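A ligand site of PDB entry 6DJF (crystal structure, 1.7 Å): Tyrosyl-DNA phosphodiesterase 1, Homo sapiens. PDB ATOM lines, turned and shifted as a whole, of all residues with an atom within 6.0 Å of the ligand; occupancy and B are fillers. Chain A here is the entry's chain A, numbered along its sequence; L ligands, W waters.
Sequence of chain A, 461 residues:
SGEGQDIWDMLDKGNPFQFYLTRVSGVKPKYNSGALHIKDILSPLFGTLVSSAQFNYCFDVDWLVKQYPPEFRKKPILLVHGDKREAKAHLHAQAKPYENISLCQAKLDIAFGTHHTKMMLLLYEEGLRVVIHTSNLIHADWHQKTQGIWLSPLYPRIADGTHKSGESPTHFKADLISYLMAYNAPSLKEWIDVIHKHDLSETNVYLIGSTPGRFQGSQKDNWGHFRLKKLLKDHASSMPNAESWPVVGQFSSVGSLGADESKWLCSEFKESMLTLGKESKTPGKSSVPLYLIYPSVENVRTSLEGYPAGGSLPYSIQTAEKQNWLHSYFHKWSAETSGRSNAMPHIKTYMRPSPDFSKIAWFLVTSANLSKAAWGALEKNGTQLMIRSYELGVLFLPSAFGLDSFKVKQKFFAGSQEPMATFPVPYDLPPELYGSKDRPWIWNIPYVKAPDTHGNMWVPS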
ATOM      1  N   ASN A  56      23.949   9.226   0.397  1.00  0.00           N
ATOM      2  CA  ASN A  56      23.981  10.400  -0.455  1.00  0.00           C
ATOM      3  C   ASN A  56      25.230  11.223  -0.199  1.00  0.00           C
ATOM      4  O   ASN A  56      26.125  10.847   0.564  1.00  0.00           O
ATOM      5  CB  ASN A  56      22.708  11.233  -0.256  1.00  0.00           C
ATOM      6  CG  ASN A  56      22.211  11.808  -1.581  1.00  0.00           C
ATOM      7  OD1 ASN A  56      22.832  12.710  -2.119  1.00  0.00           O
ATOM      8  ND2 ASN A  56      21.135  11.255  -2.119  1.00  0.00           N
ATOM      9  N   TYR A  57      25.284  12.358  -0.886  1.00  0.00           N
ATOM     10  CA  TYR A  57      26.360  13.338  -0.786  1.00  0.00           C
ATOM     11  C   TYR A  57      25.933  14.537   0.065  1.00  0.00           C
ATOM     12  O   TYR A  57      26.575  14.852   1.072  1.00  0.00           O
ATOM     13  CB  TYR A  57      26.769  13.786  -2.193  1.00  0.00           C
ATOM     14  CG  TYR A  57      27.828  14.856  -2.207  1.00  0.00           C
ATOM     15  CD1 TYR A  57      29.128  14.565  -1.811  1.00  0.00           C
ATOM     16  CD2 TYR A  57      27.526  16.143  -2.608  1.00  0.00           C
ATOM     17  CE1 TYR A  57      30.098  15.554  -1.809  1.00  0.00           C
ATOM     18  CE2 TYR A  57      28.474  17.134  -2.600  1.00  0.00           C
ATOM     19  CZ  TYR A  57      29.765  16.834  -2.214  1.00  0.00           C
ATOM     20  OH  TYR A  57      30.719  17.833  -2.227  1.00  0.00           O
ATOM     21  N   HIS A 115      31.928  10.768  -1.244  1.00  0.00           N
ATOM     22  CA  HIS A 115      30.873   9.761  -1.218  1.00  0.00           C
ATOM     23  C   HIS A 115      29.730  10.245  -2.108  1.00  0.00           C
ATOM     24  O   HIS A 115      28.858  10.997  -1.656  1.00  0.00           O
ATOM     25  CB  HIS A 115      30.387   9.502   0.204  1.00  0.00           C
ATOM     26  CG  HIS A 115      29.368   8.414   0.289  1.00  0.00           C
ATOM     27  ND1 HIS A 115      28.016   8.660   0.285  1.00  0.00           N
ATOM     28  CD2 HIS A 115      29.509   7.061   0.338  1.00  0.00           C
ATOM     29  CE1 HIS A 115      27.365   7.503   0.349  1.00  0.00           C
ATOM     30  NE2 HIS A 115      28.250   6.518   0.382  1.00  0.00           N
ATOM     31  N   HIS A 116      29.705   9.782  -3.360  1.00  0.00           N
ATOM     32  CA  HIS A 116      28.746  10.258  -4.360  1.00  0.00           C
ATOM     33  C   HIS A 116      27.573   9.316  -4.575  1.00  0.00           C
ATOM     34  O   HIS A 116      26.586   9.720  -5.215  1.00  0.00           O
ATOM     35  CB  HIS A 116      29.437  10.486  -5.703  1.00  0.00           C
ATOM     36  CG  HIS A 116      30.231  11.758  -5.778  1.00  0.00           C
ATOM     37  ND1 HIS A 116      31.351  11.880  -6.587  1.00  0.00           N
ATOM     38  CD2 HIS A 116      30.081  12.953  -5.164  1.00  0.00           C
ATOM     39  CE1 HIS A 116      31.833  13.106  -6.469  1.00  0.00           C
ATOM     40  NE2 HIS A 116      31.098  13.771  -5.597  1.00  0.00           N
ATOM     41  N   LYS A 118      24.180   7.509  -4.510  1.00  0.00           N
ATOM     42  CA  LYS A 118      22.820   7.924  -4.153  1.00  0.00           C
ATOM     43  C   LYS A 118      21.914   6.700  -4.208  1.00  0.00           C
ATOM     44  O   LYS A 118      21.637   6.158  -5.288  1.00  0.00           O
ATOM     45  CB  LYS A 118      22.374   9.056  -5.074  1.00  0.00           C
ATOM     46  CG  LYS A 118      23.338  10.216  -4.879  1.00  0.00           C
ATOM     47  CD  LYS A 118      22.995  11.411  -5.655  1.00  0.00           C
ATOM     48  CE  LYS A 118      23.985  12.498  -5.323  1.00  0.00           C
ATOM     49  NZ  LYS A 118      25.327  12.183  -5.834  1.00  0.00           N
ATOM     50  N   THR A 134      20.081   9.599  -8.753  1.00  0.00           N
ATOM     51  CA  THR A 134      21.124  10.577  -9.003  1.00  0.00           C
ATOM     52  C   THR A 134      20.968  11.888  -8.227  1.00  0.00           C
ATOM     53  O   THR A 134      21.831  12.766  -8.358  1.00  0.00           O
ATOM     54  CB  THR A 134      21.228  10.921 -10.513  1.00  0.00           C
ATOM     55  OG1 THR A 134      20.006  11.497 -10.986  1.00  0.00           O
ATOM     56  CG2 THR A 134      21.490   9.684 -11.342  1.00  0.00           C
ATOM     57  N   SER A 135      19.943  12.028  -7.389  1.00  0.00           N
ATOM     58  CA  SER A 135      19.648  13.302  -6.734  1.00  0.00           C
ATOM     59  C   SER A 135      20.204  13.381  -5.323  1.00  0.00           C
ATOM     60  O   SER A 135      20.114  12.423  -4.539  1.00  0.00           O
ATOM     61  CB  SER A 135      18.138  13.535  -6.639  1.00  0.00           C
ATOM     62  OG  SER A 135      17.525  13.448  -7.912  1.00  0.00           O
ATOM     63  N   ASN A 136      20.733  14.550  -4.987  1.00  0.00           N
ATOM     64  CA  ASN A 136      20.992  14.895  -3.585  1.00  0.00           C
ATOM     65  C   ASN A 136      19.679  15.023  -2.825  1.00  0.00           C
ATOM     66  O   ASN A 136      18.613  15.232  -3.411  1.00  0.00           O
ATOM     67  CB  ASN A 136      21.806  16.194  -3.503  1.00  0.00           C
ATOM     68  CG  ASN A 136      23.204  16.029  -4.039  1.00  0.00           C
ATOM     69  OD1 ASN A 136      24.084  15.479  -3.360  1.00  0.00           O
ATOM     70  ND2 ASN A 136      23.433  16.479  -5.265  1.00  0.00           N
ATOM     71  N   ASP A 141      17.386  19.676  -5.832  1.00  0.00           N
ATOM     72  CA  ASP A 141      17.707  18.580  -6.731  1.00  0.00           C
ATOM     73  C   ASP A 141      16.463  17.861  -7.251  1.00  0.00           C
ATOM     74  O   ASP A 141      16.572  17.127  -8.235  1.00  0.00           O
ATOM     75  CB  ASP A 141      18.638  17.562  -6.044  1.00  0.00           C
ATOM     76  CG  ASP A 141      20.112  17.828  -6.365  1.00  0.00           C
ATOM     77  OD1 ASP A 141      20.504  19.013  -6.464  1.00  0.00           O
ATOM     78  OD2 ASP A 141      20.863  16.861  -6.568  1.00  0.00           O
ATOM     79  N   SER A 252      27.347  15.752 -15.386  1.00  0.00           N
ATOM     80  CA  SER A 252      27.118  17.094 -14.838  1.00  0.00           C
ATOM     81  C   SER A 252      28.392  17.731 -14.300  1.00  0.00           C
ATOM     82  O   SER A 252      28.360  18.886 -13.860  1.00  0.00           O
ATOM     83  CB  SER A 252      26.044  17.026 -13.746  1.00  0.00           C
ATOM     84  OG  SER A 252      26.470  16.276 -12.638  1.00  0.00           O
ATOM     85  N   GLY A 311      25.126  26.202 -10.313  1.00  0.00           N
ATOM     86  CA  GLY A 311      25.666  25.848  -9.017  1.00  0.00           C
ATOM     87  C   GLY A 311      25.822  24.348  -8.844  1.00  0.00           C
ATOM     88  O   GLY A 311      26.602  23.919  -7.990  1.00  0.00           O
ATOM     89  N   SER A 312      25.099  23.562  -9.642  1.00  0.00           N
ATOM     90  CA  SER A 312      25.146  22.099  -9.593  1.00  0.00           C
ATOM     91  C   SER A 312      25.872  21.509 -10.794  1.00  0.00           C
ATOM     92  O   SER A 312      25.736  20.308 -11.066  1.00  0.00           O
ATOM     93  CB  SER A 312      23.736  21.533  -9.484  1.00  0.00           C
ATOM     94  OG  SER A 312      23.118  21.948  -8.282  1.00  0.00           O
ATOM     95  N   LEU A 313      26.661  22.310 -11.510  1.00  0.00           N
ATOM     96  CA  LEU A 313      27.478  21.876 -12.649  1.00  0.00           C
ATOM     97  C   LEU A 313      28.885  22.405 -12.376  1.00  0.00           C
ATOM     98  O   LEU A 313      29.292  23.422 -12.954  1.00  0.00           O
ATOM     99  CB  LEU A 313      26.912  22.400 -13.968  1.00  0.00           C
ATOM    100  CG  LEU A 313      25.507  21.946 -14.395  1.00  0.00           C
ATOM    101  CD1 LEU A 313      24.872  22.922 -15.395  1.00  0.00           C
ATOM    102  CD2 LEU A 313      25.532  20.544 -14.998  1.00  0.00           C
ATOM    103  N   PRO A 314      29.633  21.762 -11.474  1.00  0.00           N
ATOM    104  CA  PRO A 314      30.822  22.402 -10.872  1.00  0.00           C
ATOM    105  C   PRO A 314      32.119  22.177 -11.647  1.00  0.00           C
ATOM    106  O   PRO A 314      33.122  21.698 -11.110  1.00  0.00           O
ATOM    107  CB  PRO A 314      30.865  21.754  -9.481  1.00  0.00           C
ATOM    108  CG  PRO A 314      30.301  20.386  -9.702  1.00  0.00           C
ATOM    109  CD  PRO A 314      29.263  20.513 -10.794  1.00  0.00           C
ATOM    110  N   HIS A 346      21.230  16.621 -13.845  1.00  0.00           N
ATOM    111  CA  HIS A 346      22.080  16.114 -12.793  1.00  0.00           C
ATOM    112  C   HIS A 346      22.176  14.599 -12.860  1.00  0.00           C
ATOM    113  O   HIS A 346      23.002  13.997 -12.157  1.00  0.00           O
ATOM    114  CB  HIS A 346      21.555  16.597 -11.432  1.00  0.00           C
ATOM    115  CG  HIS A 346      22.496  16.368 -10.294  1.00  0.00           C
ATOM    116  ND1 HIS A 346      22.416  15.263  -9.468  1.00  0.00           N
ATOM    117  CD2 HIS A 346      23.521  17.116  -9.819  1.00  0.00           C
ATOM    118  CE1 HIS A 346      23.364  15.328  -8.545  1.00  0.00           C
ATOM    119  NE2 HIS A 346      24.046  16.450  -8.729  1.00  0.00           N
ATOM    120  N   LYS A 348      23.491  11.205 -14.700  1.00  0.00           N
ATOM    121  CA  LYS A 348      24.648  10.860 -15.517  1.00  0.00           C
ATOM    122  C   LYS A 348      24.297   9.555 -16.208  1.00  0.00           C
ATOM    123  O   LYS A 348      23.747   8.655 -15.572  1.00  0.00           O
ATOM    124  CB  LYS A 348      25.936  10.657 -14.701  1.00  0.00           C
ATOM    125  CG  LYS A 348      26.400  11.892 -13.916  1.00  0.00           C
ATOM    126  CD  LYS A 348      25.765  11.963 -12.516  1.00  0.00           C
ATOM    127  CE  LYS A 348      26.393  13.070 -11.692  1.00  0.00           C
ATOM    128  NZ  LYS A 348      25.403  13.784 -10.852  1.00  0.00           N
ATOM    129  N   SER A 367      25.739   7.612 -10.627  1.00  0.00           N
ATOM    130  CA  SER A 367      26.208   8.837 -10.003  1.00  0.00           C
ATOM    131  C   SER A 367      27.551   9.315 -10.564  1.00  0.00           C
ATOM    132  O   SER A 367      27.928  10.471 -10.329  1.00  0.00           O
ATOM    133  CB  SER A 367      26.346   8.642  -8.491  1.00  0.00           C
ATOM    134  OG  SER A 367      27.299   7.634  -8.185  1.00  0.00           O
ATOM    135  N   ASN A 369      30.380  10.902 -12.559  1.00  0.00           N
ATOM    136  CA  ASN A 369      30.687  11.929 -13.551  1.00  0.00           C
ATOM    137  C   ASN A 369      31.901  11.528 -14.384  1.00  0.00           C
ATOM    138  O   ASN A 369      32.480  10.447 -14.209  1.00  0.00           O
ATOM    139  CB  ASN A 369      30.903  13.269 -12.841  1.00  0.00           C
ATOM    140  CG  ASN A 369      29.614  14.002 -12.605  1.00  0.00           C
ATOM    141  OD1 ASN A 369      28.793  14.092 -13.507  1.00  0.00           O
ATOM    142  ND2 ASN A 369      29.429  14.530 -11.403  1.00  0.00           N
ATOM    143  N   TRP A 443      31.587  27.110 -13.743  1.00  0.00           N
ATOM    144  CA  TRP A 443      30.721  27.677 -12.711  1.00  0.00           C
ATOM    145  C   TRP A 443      31.348  28.846 -11.958  1.00  0.00           C
ATOM    146  O   TRP A 443      30.608  29.619 -11.336  1.00  0.00           O
ATOM    147  CB  TRP A 443      30.277  26.628 -11.690  1.00  0.00           C
ATOM    148  CG  TRP A 443      31.314  26.126 -10.714  1.00  0.00           C
ATOM    149  CD1 TRP A 443      32.668  26.077 -10.891  1.00  0.00           C
ATOM    150  CD2 TRP A 443      31.062  25.595  -9.405  1.00  0.00           C
ATOM    151  NE1 TRP A 443      33.271  25.552  -9.771  1.00  0.00           N
ATOM    152  CE2 TRP A 443      32.313  25.250  -8.850  1.00  0.00           C
ATOM    153  CE3 TRP A 443      29.895  25.380  -8.656  1.00  0.00           C
ATOM    154  CZ2 TRP A 443      32.426  24.691  -7.563  1.00  0.00           C
ATOM    155  CZ3 TRP A 443      30.022  24.838  -7.380  1.00  0.00           C
ATOM    156  CH2 TRP A 443      31.276  24.502  -6.855  1.00  0.00           C
HETATM  157  C1  LIG L   1      27.719  21.338  -6.782  1.00  0.00           C
HETATM  158  C2  LIG L   1      27.694  18.926  -6.528  1.00  0.00           C
HETATM  159  C3  LIG L   1      26.986  15.190  -6.372  1.00  0.00           C
HETATM  160  C4  LIG L   1      27.673  16.544  -6.258  1.00  0.00           C
HETATM  161  C5  LIG L   1      28.979  16.646  -5.805  1.00  0.00           C
HETATM  162  C6  LIG L   1      28.984  18.955  -6.054  1.00  0.00           C
HETATM  163  C7  LIG L   1      29.664  20.190  -5.941  1.00  0.00           C
HETATM  164  C8  LIG L   1      31.096  20.241  -5.414  1.00  0.00           C
HETATM  165  C9  LIG L   1      29.031  21.370  -6.302  1.00  0.00           C
HETATM  166  C10 LIG L   1      27.041  20.126  -6.901  1.00  0.00           C
HETATM  167  C11 LIG L   1      27.008  17.710  -6.635  1.00  0.00           C
HETATM  168  N1  LIG L   1      29.603  17.816  -5.702  1.00  0.00           N
HETATM  169  O1  LIG L   1      25.742  15.132  -6.528  1.00  0.00           O
HETATM  170  O2  LIG L   1      27.671  14.132  -6.335  1.00  0.00           O
HETATM  171  O3  LIG L   1      31.873  19.259  -5.615  1.00  0.00           O
HETATM  172  O4  LIG L   1      31.502  21.259  -4.794  1.00  0.00           O
HETATM  173  O5  LIG L   1      25.890  17.678  -7.047  1.00  0.00           O
HETATM  174  O   HOH W   1      32.171  16.396  -5.112  1.00  0.00           O
HETATM  175  O   HOH W   2      27.194  15.182  -9.343  1.00  0.00           O
HETATM  176  O   HOH W   3      27.371  12.395  -8.281  1.00  0.00           O
HETATM  177  O   HOH W   4      29.822  20.611  -2.599  1.00  0.00           O
HETATM  178  O   HOH W   5      23.194  19.553  -6.706  1.00  0.00           O
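The backbone carbonyl oxygen (O) of His 346 sits at hydrogen-bond distance from the side-chain amino group (NZ) of Lys 348 (2.7 Å). A ring nitrogen (ND1) of His 346 sits at hydrogen-bond distance from the backbone carbonyl oxygen (O) of Thr 134. O of His 116 sits at hydrogen-bond distance from NZ of Lys 118, 2.8 Å away. The backbone NH (N) of Asn 136 is in hydrogen-bond range of the side-chain carboxylate (OD2) of Asp 141. The side-chain amide oxygen (OD1) of Asn 136 sits close to the side-chain amide oxygen (OD1) of Asn 56, at 3.3 Å.
An oxygen (O5) of the ligand sits at hydrogen-bond distance from a ring nitrogen (NE2) of His 346 (2.8 Å). O1 of the ligand is in hydrogen-bond range of ND2 of Asn 136. An oxygen (O1) of the ligand lies within salt-bridge range of the side-chain amino group (NZ) of Lys 118 (3.1 Å).
Water W3 lies within hydrogen-bond range of an oxygen (O2) of the ligand (2.6 Å), the backbone carbonyl oxygen (O) of Ser 367 (2.9 Å) and the side-chain amino group (NZ) of Lys 118 (3.2 Å). Water W4 lies within hydrogen-bond range of O4 of the ligand and OH of Tyr 57. Water W1 lies within hydrogen-bond range of NE2 of His 116 (2.9 Å) and O3 of the ligand (2.9 Å). Water W2 lies within hydrogen-bond range of the side-chain amino group of Lys 348 (2.7 Å), the side-chain amide nitrogen of Asn 369 (3.1 Å), an oxygen (O1) of the ligand (3.2 Å) and a ring nitrogen (NE2) of His 346 (3.4 Å). Water W5 lies within hydrogen-bond range of the side-chain carboxylate (OD1) of Asp 141 (2.8 Å), the side-chain hydroxyl (OG) of Ser 312 (2.9 Å), an oxygen (O5) of the ligand (3.3 Å) and the side-chain amide nitrogen (ND2) of Asn 136 (3.4 Å).
Tyr 57 touches the ligand. His 116 touches the ligand (CD2 to O2, 2.9 Å). Gly 311 touches the ligand (O to C1, 3.1 Å). Ser 312 touches the ligand. CB of Pro 314 touches C9 of the ligand, at 3.7 Å. CZ3 of Trp 443 touches C9 of the ligand (3.8 Å). Hydrophobic or aromatic side chains that line the ligand: Tyr 57, His 116, Pro 314, His 346 and Trp 443. Nine residues have an atom within 4 Å of the ligand: Tyr 57, His 116, Lys 118, Asn 136, Gly 311, Ser 312, Pro 314, His 346 and Trp 443.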
